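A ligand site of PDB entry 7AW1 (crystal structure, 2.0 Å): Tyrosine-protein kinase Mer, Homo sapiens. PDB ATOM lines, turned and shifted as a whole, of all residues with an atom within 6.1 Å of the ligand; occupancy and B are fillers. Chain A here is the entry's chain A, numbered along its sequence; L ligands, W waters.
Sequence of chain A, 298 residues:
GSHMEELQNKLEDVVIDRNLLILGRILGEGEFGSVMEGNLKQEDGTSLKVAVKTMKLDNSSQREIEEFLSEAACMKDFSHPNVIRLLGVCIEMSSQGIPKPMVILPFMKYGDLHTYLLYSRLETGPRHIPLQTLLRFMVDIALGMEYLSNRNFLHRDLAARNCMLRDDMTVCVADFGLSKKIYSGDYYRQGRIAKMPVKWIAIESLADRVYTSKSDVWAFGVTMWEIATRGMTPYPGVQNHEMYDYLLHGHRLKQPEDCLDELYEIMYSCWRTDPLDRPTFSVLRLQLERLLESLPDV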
ATOM      1  N   LEU A  27      12.764  19.082  11.260  1.00  0.00           N
ATOM      2  CA  LEU A  27      13.238  18.572  12.550  1.00  0.00           C
ATOM      3  C   LEU A  27      12.534  17.258  12.933  1.00  0.00           C
ATOM      4  O   LEU A  27      13.119  16.425  13.633  1.00  0.00           O
ATOM      5  CB  LEU A  27      13.000  19.621  13.674  1.00  0.00           C
ATOM      6  CG  LEU A  27      13.591  21.027  13.514  1.00  0.00           C
ATOM      7  CD1 LEU A  27      12.945  21.993  14.494  1.00  0.00           C
ATOM      8  CD2 LEU A  27      15.101  21.030  13.714  1.00  0.00           C
ATOM      9  N   VAL A  35       7.408  19.449  11.729  1.00  0.00           N
ATOM     10  CA  VAL A  35       8.031  20.486  12.547  1.00  0.00           C
ATOM     11  C   VAL A  35       9.345  20.867  11.838  1.00  0.00           C
ATOM     12  O   VAL A  35      10.151  19.990  11.511  1.00  0.00           O
ATOM     13  CB  VAL A  35       8.259  20.076  14.037  1.00  0.00           C
ATOM     14  CG1 VAL A  35       8.905  21.209  14.834  1.00  0.00           C
ATOM     15  CG2 VAL A  35       6.948  19.651  14.698  1.00  0.00           C
ATOM     16  N   ALA A  51      10.285  27.649  15.753  1.00  0.00           N
ATOM     17  CA  ALA A  51       9.905  26.304  15.334  1.00  0.00           C
ATOM     18  C   ALA A  51       8.576  26.484  14.574  1.00  0.00           C
ATOM     19  O   ALA A  51       7.694  27.195  15.044  1.00  0.00           O
ATOM     20  CB  ALA A  51       9.696  25.399  16.536  1.00  0.00           C
ATOM     21  N   VAL A  52       8.455  25.884  13.385  1.00  0.00           N
ATOM     22  CA  VAL A  52       7.242  26.003  12.577  1.00  0.00           C
ATOM     23  C   VAL A  52       6.567  24.631  12.421  1.00  0.00           C
ATOM     24  O   VAL A  52       7.161  23.696  11.860  1.00  0.00           O
ATOM     25  CB  VAL A  52       7.494  26.676  11.195  1.00  0.00           C
ATOM     26  CG1 VAL A  52       6.187  26.876  10.439  1.00  0.00           C
ATOM     27  CG2 VAL A  52       8.245  27.999  11.348  1.00  0.00           C
ATOM     28  N   LYS A  53       5.309  24.532  12.906  1.00  0.00           N
ATOM     29  CA  LYS A  53       4.522  23.297  12.808  1.00  0.00           C
ATOM     30  C   LYS A  53       3.471  23.435  11.705  1.00  0.00           C
ATOM     31  O   LYS A  53       2.657  24.348  11.745  1.00  0.00           O
ATOM     32  CB  LYS A  53       3.898  22.926  14.160  1.00  0.00           C
ATOM     33  CG  LYS A  53       3.524  21.455  14.255  1.00  0.00           C
ATOM     34  CD  LYS A  53       2.033  21.232  14.220  1.00  0.00           C
ATOM     35  CE  LYS A  53       1.697  19.773  14.426  1.00  0.00           C
ATOM     36  NZ  LYS A  53       0.390  19.591  15.109  1.00  0.00           N
ATOM     37  N   MET A  75      -5.097  30.599  22.233  1.00  0.00           N
ATOM     38  CA  MET A  75      -3.758  30.210  22.680  1.00  0.00           C
ATOM     39  C   MET A  75      -2.793  31.394  22.757  1.00  0.00           C
ATOM     40  O   MET A  75      -1.990  31.454  23.692  1.00  0.00           O
ATOM     41  CB  MET A  75      -3.202  29.141  21.753  1.00  0.00           C
ATOM     42  CG  MET A  75      -2.083  28.353  22.356  1.00  0.00           C
ATOM     43  SD  MET A  75      -1.311  27.261  21.149  1.00  0.00           S
ATOM     44  CE  MET A  75      -2.816  26.582  20.310  1.00  0.00           C
ATOM     45  N   PHE A  78      -3.060  33.477  25.988  1.00  0.00           N
ATOM     46  CA  PHE A  78      -2.462  32.914  27.223  1.00  0.00           C
ATOM     47  C   PHE A  78      -1.155  33.667  27.520  1.00  0.00           C
ATOM     48  O   PHE A  78      -0.393  33.954  26.604  1.00  0.00           O
ATOM     49  CB  PHE A  78      -2.117  31.425  27.065  1.00  0.00           C
ATOM     50  CG  PHE A  78      -3.238  30.427  26.890  1.00  0.00           C
ATOM     51  CD1 PHE A  78      -4.518  30.690  27.372  1.00  0.00           C
ATOM     52  CD2 PHE A  78      -3.002  29.188  26.310  1.00  0.00           C
ATOM     53  CE1 PHE A  78      -5.535  29.746  27.246  1.00  0.00           C
ATOM     54  CE2 PHE A  78      -4.027  28.246  26.189  1.00  0.00           C
ATOM     55  CZ  PHE A  78      -5.288  28.534  26.652  1.00  0.00           C
ATOM     56  N   VAL A  83       3.585  28.117  30.294  1.00  0.00           N
ATOM     57  CA  VAL A  83       2.719  27.731  29.177  1.00  0.00           C
ATOM     58  C   VAL A  83       3.467  28.228  27.923  1.00  0.00           C
ATOM     59  O   VAL A  83       3.885  29.398  27.920  1.00  0.00           O
ATOM     60  CB  VAL A  83       1.294  28.345  29.303  1.00  0.00           C
ATOM     61  CG1 VAL A  83       0.436  28.028  28.088  1.00  0.00           C
ATOM     62  CG2 VAL A  83       0.600  27.884  30.597  1.00  0.00           C
ATOM     63  N   ILE A  84       3.656  27.369  26.886  1.00  0.00           N
ATOM     64  CA  ILE A  84       4.389  27.758  25.650  1.00  0.00           C
ATOM     65  C   ILE A  84       3.708  28.990  24.989  1.00  0.00           C
ATOM     66  O   ILE A  84       2.473  29.062  24.981  1.00  0.00           O
ATOM     67  CB  ILE A  84       4.577  26.577  24.641  1.00  0.00           C
ATOM     68  CG1 ILE A  84       5.672  26.903  23.573  1.00  0.00           C
ATOM     69  CG2 ILE A  84       3.238  26.152  23.976  1.00  0.00           C
ATOM     70  CD1 ILE A  84       6.332  25.681  22.913  1.00  0.00           C
ATOM     71  N   VAL A 103       1.759  26.903  12.422  1.00  0.00           N
ATOM     72  CA  VAL A 103       1.780  27.535  13.754  1.00  0.00           C
ATOM     73  C   VAL A 103       3.267  27.859  14.129  1.00  0.00           C
ATOM     74  O   VAL A 103       4.168  27.044  13.883  1.00  0.00           O
ATOM     75  CB  VAL A 103       0.943  26.804  14.858  1.00  0.00           C
ATOM     76  CG1 VAL A 103       0.191  25.577  14.323  1.00  0.00           C
ATOM     77  CG2 VAL A 103       1.731  26.475  16.106  1.00  0.00           C
ATOM     78  N   LEU A 105       6.164  29.156  16.907  1.00  0.00           N
ATOM     79  CA  LEU A 105       6.531  29.148  18.320  1.00  0.00           C
ATOM     80  C   LEU A 105       8.017  29.461  18.515  1.00  0.00           C
ATOM     81  O   LEU A 105       8.787  29.225  17.574  1.00  0.00           O
ATOM     82  CB  LEU A 105       6.219  27.771  18.925  1.00  0.00           C
ATOM     83  CG  LEU A 105       4.777  27.341  18.727  1.00  0.00           C
ATOM     84  CD1 LEU A 105       4.721  26.133  17.912  1.00  0.00           C
ATOM     85  CD2 LEU A 105       4.034  27.243  20.015  1.00  0.00           C
ATOM     86  N   PRO A 106       8.463  29.913  19.721  1.00  0.00           N
ATOM     87  CA  PRO A 106       9.910  30.155  19.908  1.00  0.00           C
ATOM     88  C   PRO A 106      10.673  28.841  19.858  1.00  0.00           C
ATOM     89  O   PRO A 106      10.144  27.802  20.286  1.00  0.00           O
ATOM     90  CB  PRO A 106       9.996  30.796  21.303  1.00  0.00           C
ATOM     91  CG  PRO A 106       8.582  31.193  21.651  1.00  0.00           C
ATOM     92  CD  PRO A 106       7.713  30.205  20.951  1.00  0.00           C
ATOM     93  N   PHE A 107      11.895  28.871  19.285  1.00  0.00           N
ATOM     94  CA  PHE A 107      12.701  27.672  19.167  1.00  0.00           C
ATOM     95  C   PHE A 107      13.343  27.324  20.500  1.00  0.00           C
ATOM     96  O   PHE A 107      13.969  28.184  21.135  1.00  0.00           O
ATOM     97  CB  PHE A 107      13.777  27.837  18.064  1.00  0.00           C
ATOM     98  CG  PHE A 107      14.566  26.577  17.813  1.00  0.00           C
ATOM     99  CD1 PHE A 107      14.066  25.570  16.993  1.00  0.00           C
ATOM    100  CD2 PHE A 107      15.803  26.371  18.432  1.00  0.00           C
ATOM    101  CE1 PHE A 107      14.781  24.383  16.805  1.00  0.00           C
ATOM    102  CE2 PHE A 107      16.529  25.198  18.220  1.00  0.00           C
ATOM    103  CZ  PHE A 107      16.009  24.213  17.400  1.00  0.00           C
ATOM    104  N   MET A 108      13.193  26.056  20.927  1.00  0.00           N
ATOM    105  CA  MET A 108      13.773  25.580  22.175  1.00  0.00           C
ATOM    106  C   MET A 108      14.775  24.467  21.881  1.00  0.00           C
ATOM    107  O   MET A 108      14.394  23.354  21.530  1.00  0.00           O
ATOM    108  CB  MET A 108      12.667  25.176  23.173  1.00  0.00           C
ATOM    109  CG  MET A 108      11.806  26.354  23.576  1.00  0.00           C
ATOM    110  SD  MET A 108      10.437  25.875  24.595  1.00  0.00           S
ATOM    111  CE  MET A 108       9.429  27.300  24.462  1.00  0.00           C
ATOM    112  N   LYS A 109      16.072  24.824  21.937  1.00  0.00           N
ATOM    113  CA  LYS A 109      17.184  23.944  21.618  1.00  0.00           C
ATOM    114  C   LYS A 109      17.217  22.636  22.423  1.00  0.00           C
ATOM    115  O   LYS A 109      17.674  21.628  21.896  1.00  0.00           O
ATOM    116  CB  LYS A 109      18.543  24.684  21.704  1.00  0.00           C
ATOM    117  CG  LYS A 109      18.968  25.141  23.096  1.00  0.00           C
ATOM    118  CD  LYS A 109      20.300  25.880  23.034  1.00  0.00           C
ATOM    119  CE  LYS A 109      20.897  26.137  24.383  1.00  0.00           C
ATOM    120  NZ  LYS A 109      22.346  26.487  24.287  1.00  0.00           N
ATOM    121  N   TYR A 110      16.703  22.624  23.677  1.00  0.00           N
ATOM    122  CA  TYR A 110      16.704  21.418  24.505  1.00  0.00           C
ATOM    123  C   TYR A 110      15.567  20.432  24.158  1.00  0.00           C
ATOM    124  O   TYR A 110      15.662  19.281  24.558  1.00  0.00           O
ATOM    125  CB  TYR A 110      16.734  21.735  26.039  1.00  0.00           C
ATOM    126  CG  TYR A 110      18.052  22.347  26.481  1.00  0.00           C
ATOM    127  CD1 TYR A 110      19.268  21.722  26.191  1.00  0.00           C
ATOM    128  CD2 TYR A 110      18.085  23.569  27.130  1.00  0.00           C
ATOM    129  CE1 TYR A 110      20.481  22.310  26.541  1.00  0.00           C
ATOM    130  CE2 TYR A 110      19.298  24.170  27.490  1.00  0.00           C
ATOM    131  CZ  TYR A 110      20.492  23.535  27.193  1.00  0.00           C
ATOM    132  OH  TYR A 110      21.690  24.105  27.546  1.00  0.00           O
ATOM    133  N   GLY A 111      14.551  20.890  23.419  1.00  0.00           N
ATOM    134  CA  GLY A 111      13.440  20.034  22.977  1.00  0.00           C
ATOM    135  C   GLY A 111      12.464  19.578  24.059  1.00  0.00           C
ATOM    136  O   GLY A 111      12.308  20.246  25.087  1.00  0.00           O
ATOM    137  N   ASP A 112      11.753  18.460  23.786  1.00  0.00           N
ATOM    138  CA  ASP A 112      10.734  17.906  24.698  1.00  0.00           C
ATOM    139  C   ASP A 112      11.347  17.262  25.947  1.00  0.00           C
ATOM    140  O   ASP A 112      12.484  16.765  25.910  1.00  0.00           O
ATOM    141  CB  ASP A 112       9.765  16.957  23.956  1.00  0.00           C
ATOM    142  CG  ASP A 112      10.317  15.555  23.717  1.00  0.00           C
ATOM    143  OD1 ASP A 112      11.019  15.348  22.696  1.00  0.00           O
ATOM    144  OD2 ASP A 112      10.022  14.651  24.545  1.00  0.00           O
ATOM    145  N   LEU A 148      -3.960  27.316  33.377  1.00  0.00           N
ATOM    146  CA  LEU A 148      -4.933  26.829  32.405  1.00  0.00           C
ATOM    147  C   LEU A 148      -6.262  26.398  33.029  1.00  0.00           C
ATOM    148  O   LEU A 148      -7.322  26.826  32.542  1.00  0.00           O
ATOM    149  CB  LEU A 148      -4.344  25.699  31.540  1.00  0.00           C
ATOM    150  CG  LEU A 148      -3.093  26.028  30.669  1.00  0.00           C
ATOM    151  CD1 LEU A 148      -2.606  24.785  29.946  1.00  0.00           C
ATOM    152  CD2 LEU A 148      -3.396  27.149  29.634  1.00  0.00           C
ATOM    153  N   PHE A 153      -9.775  25.958  30.910  1.00  0.00           N
ATOM    154  CA  PHE A 153      -9.227  25.342  29.718  1.00  0.00           C
ATOM    155  C   PHE A 153      -8.789  23.903  30.024  1.00  0.00           C
ATOM    156  O   PHE A 153      -8.204  23.651  31.087  1.00  0.00           O
ATOM    157  CB  PHE A 153      -8.064  26.181  29.189  1.00  0.00           C
ATOM    158  CG  PHE A 153      -7.669  25.905  27.767  1.00  0.00           C
ATOM    159  CD1 PHE A 153      -8.318  26.545  26.706  1.00  0.00           C
ATOM    160  CD2 PHE A 153      -6.624  25.037  27.476  1.00  0.00           C
ATOM    161  CE1 PHE A 153      -7.932  26.302  25.378  1.00  0.00           C
ATOM    162  CE2 PHE A 153      -6.247  24.787  26.156  1.00  0.00           C
ATOM    163  CZ  PHE A 153      -6.905  25.422  25.117  1.00  0.00           C
ATOM    164  N   LEU A 154      -9.103  22.973  29.116  1.00  0.00           N
ATOM    165  CA  LEU A 154      -8.758  21.553  29.248  1.00  0.00           C
ATOM    166  C   LEU A 154      -7.615  21.210  28.290  1.00  0.00           C
ATOM    167  O   LEU A 154      -7.666  21.620  27.125  1.00  0.00           O
ATOM    168  CB  LEU A 154      -9.984  20.653  28.974  1.00  0.00           C
ATOM    169  CG  LEU A 154     -11.200  20.801  29.907  1.00  0.00           C
ATOM    170  CD1 LEU A 154     -12.326  19.860  29.491  1.00  0.00           C
ATOM    171  CD2 LEU A 154     -10.830  20.568  31.368  1.00  0.00           C
ATOM    172  N   HIS A 155      -6.562  20.514  28.776  1.00  0.00           N
ATOM    173  CA  HIS A 155      -5.418  20.145  27.927  1.00  0.00           C
ATOM    174  C   HIS A 155      -5.767  18.937  27.053  1.00  0.00           C
ATOM    175  O   HIS A 155      -5.590  19.006  25.833  1.00  0.00           O
ATOM    176  CB  HIS A 155      -4.137  19.904  28.763  1.00  0.00           C
ATOM    177  CG  HIS A 155      -2.882  19.778  27.938  1.00  0.00           C
ATOM    178  ND1 HIS A 155      -2.693  18.728  27.051  1.00  0.00           N
ATOM    179  CD2 HIS A 155      -1.786  20.568  27.920  1.00  0.00           C
ATOM    180  CE1 HIS A 155      -1.513  18.931  26.496  1.00  0.00           C
ATOM    181  NE2 HIS A 155      -0.928  20.027  26.982  1.00  0.00           N
ATOM    182  N   MET A 164       7.924  21.153  27.188  1.00  0.00           N
ATOM    183  CA  MET A 164       9.164  21.620  26.554  1.00  0.00           C
ATOM    184  C   MET A 164      10.111  22.255  27.575  1.00  0.00           C
ATOM    185  O   MET A 164       9.640  22.804  28.557  1.00  0.00           O
ATOM    186  CB  MET A 164       8.836  22.642  25.438  1.00  0.00           C
ATOM    187  CG  MET A 164       7.939  22.107  24.332  1.00  0.00           C
ATOM    188  SD  MET A 164       8.708  20.851  23.259  1.00  0.00           S
ATOM    189  CE  MET A 164       9.976  21.810  22.493  1.00  0.00           C
ATOM    190  N   VAL A 173       4.208  23.843  29.527  1.00  0.00           N
ATOM    191  CA  VAL A 173       3.212  22.951  28.930  1.00  0.00           C
ATOM    192  C   VAL A 173       2.966  23.359  27.468  1.00  0.00           C
ATOM    193  O   VAL A 173       2.907  24.560  27.161  1.00  0.00           O
ATOM    194  CB  VAL A 173       1.898  22.794  29.759  1.00  0.00           C
ATOM    195  CG1 VAL A 173       2.170  22.189  31.141  1.00  0.00           C
ATOM    196  CG2 VAL A 173       1.167  24.128  29.910  1.00  0.00           C
ATOM    197  N   ALA A 174       2.861  22.362  26.567  1.00  0.00           N
ATOM    198  CA  ALA A 174       2.699  22.518  25.117  1.00  0.00           C
ATOM    199  C   ALA A 174       1.847  21.356  24.563  1.00  0.00           C
ATOM    200  O   ALA A 174       1.285  20.613  25.361  1.00  0.00           O
ATOM    201  CB  ALA A 174       4.073  22.545  24.456  1.00  0.00           C
ATOM    202  N   ASP A 175       1.726  21.205  23.220  1.00  0.00           N
ATOM    203  CA  ASP A 175       0.921  20.126  22.599  1.00  0.00           C
ATOM    204  C   ASP A 175       1.258  19.964  21.115  1.00  0.00           C
ATOM    205  O   ASP A 175       0.628  20.636  20.282  1.00  0.00           O
ATOM    206  CB  ASP A 175      -0.590  20.394  22.801  1.00  0.00           C
ATOM    207  CG  ASP A 175      -1.539  19.255  22.481  1.00  0.00           C
ATOM    208  OD1 ASP A 175      -1.062  18.158  22.109  1.00  0.00           O
ATOM    209  OD2 ASP A 175      -2.775  19.461  22.608  1.00  0.00           O
ATOM    210  N   PHE A 176       2.222  19.081  20.775  1.00  0.00           N
ATOM    211  CA  PHE A 176       2.678  18.830  19.390  1.00  0.00           C
ATOM    212  C   PHE A 176       1.557  18.541  18.377  1.00  0.00           C
ATOM    213  O   PHE A 176       0.537  17.942  18.707  1.00  0.00           O
ATOM    214  CB  PHE A 176       3.722  17.702  19.352  1.00  0.00           C
ATOM    215  CG  PHE A 176       5.113  18.101  19.794  1.00  0.00           C
ATOM    216  CD1 PHE A 176       5.486  18.022  21.123  1.00  0.00           C
ATOM    217  CD2 PHE A 176       6.062  18.502  18.862  1.00  0.00           C
ATOM    218  CE1 PHE A 176       6.786  18.356  21.521  1.00  0.00           C
ATOM    219  CE2 PHE A 176       7.362  18.836  19.260  1.00  0.00           C
ATOM    220  CZ  PHE A 176       7.720  18.758  20.587  1.00  0.00           C
HETATM  221  C1  LIG L   1       5.677  22.546  17.646  1.00  0.00           C
HETATM  222  C2  LIG L   1       6.560  22.392  18.707  1.00  0.00           C
HETATM  223  C3  LIG L   1       6.116  22.550  20.007  1.00  0.00           C
HETATM  224  N1  LIG L   1       8.746  23.966  19.476  1.00  0.00           N
HETATM  225  C4  LIG L   1      -0.564  23.716  21.247  1.00  0.00           C
HETATM  226  C5  LIG L   1      -1.752  23.187  20.761  1.00  0.00           C
HETATM  227  C6  LIG L   1      -2.833  23.034  21.606  1.00  0.00           C
HETATM  228  C7  LIG L   1      -2.764  23.408  22.954  1.00  0.00           C
HETATM  229  C8  LIG L   1      -1.563  23.950  23.453  1.00  0.00           C
HETATM  230  C9  LIG L   1      -0.480  24.096  22.581  1.00  0.00           C
HETATM  231  C10 LIG L   1      -1.305  24.405  24.866  1.00  0.00           C
HETATM  232  C11 LIG L   1      -3.968  23.230  23.866  1.00  0.00           C
HETATM  233  C12 LIG L   1       8.946  22.779  18.929  1.00  0.00           C
HETATM  234  C13 LIG L   1      10.182  22.157  18.831  1.00  0.00           C
HETATM  235  C14 LIG L   1       9.859  24.550  19.948  1.00  0.00           C
HETATM  236  C15 LIG L   1      15.176  19.876  19.648  1.00  0.00           C
HETATM  237  O1  LIG L   1      12.449  20.392  18.367  1.00  0.00           O
HETATM  238  C16 LIG L   1      13.118  21.275  18.898  1.00  0.00           C
HETATM  239  C17 LIG L   1      14.630  21.158  19.076  1.00  0.00           C
HETATM  240  C18 LIG L   1      15.370  20.169  18.207  1.00  0.00           C
HETATM  241  N2  LIG L   1      12.597  22.441  19.373  1.00  0.00           N
HETATM  242  C19 LIG L   1      11.262  22.881  19.361  1.00  0.00           C
HETATM  243  N3  LIG L   1      11.111  24.089  19.928  1.00  0.00           N
HETATM  244  O2  LIG L   1       7.901  22.064  18.408  1.00  0.00           O
HETATM  245  C20 LIG L   1       4.788  22.876  20.256  1.00  0.00           C
HETATM  246  C21 LIG L   1       3.897  23.032  19.201  1.00  0.00           C
HETATM  247  C22 LIG L   1       4.356  22.860  17.892  1.00  0.00           C
HETATM  248  N4  LIG L   1       2.521  23.364  19.372  1.00  0.00           N
HETATM  249  C23 LIG L   1       1.831  23.574  20.539  1.00  0.00           C
HETATM  250  O3  LIG L   1       2.330  23.549  21.662  1.00  0.00           O
HETATM  251  N5  LIG L   1       0.503  23.839  20.314  1.00  0.00           N
HETATM  252  F1  LIG L   1      -1.406  23.408  25.758  1.00  0.00           F
HETATM  253  F2  LIG L   1      -0.069  24.909  25.041  1.00  0.00           F
HETATM  254  F3  LIG L   1      -2.150  25.364  25.265  1.00  0.00           F
HETATM  255  O   HOH W   1       0.117  23.538  17.278  1.00  0.00           O
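O of Asp 175 sits close to N5 of the ligand (3.2 Å).
The backbone NH (N) of Met 108 lies within hydrogen-bond range of a nitrogen (N3) of the ligand.
O of Met 108 lies within hydrogen-bond range of N2 of the ligand (3.0 Å).
The backbone NH (N) of Asp 175 sits at hydrogen-bond distance from an oxygen (O3) of the ligand (2.9 Å).
O of Ala 174 is in hydrogen-bond range of NE2 of His 155, 2.8 Å away.
O of Lys 53 sits at hydrogen-bond distance from N of Val 103, at 2.8 Å.
The backbone carbonyl oxygen (O) of Val 35 lies within hydrogen-bond range of the backbone NH (N) of Leu 27 (2.8 Å).
The backbone carbonyl oxygen (O) of Leu 105 is in hydrogen-bond range of the backbone NH (N) of Ala 51 (2.8 Å).
N of Phe 153 sits at hydrogen-bond distance from O of Leu 148, 3.1 Å away.
The backbone NH (N) of Ile 84 is in hydrogen-bond range of the backbone carbonyl oxygen (O) of Val 173 (2.9 Å).
Merely in contact with the ligand: Pro 106 (3.3 Å), Leu 105 (3.3 Å), Phe 176 (3.4 Å), Ala 51 (3.4 Å), Ala 174 (3.4 Å), Met 164 (3.6 Å), Phe 78 (3.6 Å), Met 75 (3.6 Å), Phe 153 (3.6 Å), His 155 (3.6 Å), Ile 84 (3.6 Å), Val 173 (3.7 Å), Phe 107 (3.7 Å), Gly 111 (3.8 Å), Lys 53 (3.8 Å), Lys 109 (3.8 Å) and Val 35 (3.8 Å).
Within 4 Å of the ligand: Val 35, Ala 51, Lys 53, Met 75, Phe 78, Ile 84, Leu 105, Pro 106, Phe 107, Met 108, Lys 109, Gly 111, Phe 153, His 155, Met 164, Val 173, Ala 174, Asp 175 and Phe 176.
Along chain A the residues within 4 Å of the ligand span positions 35 to 176.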
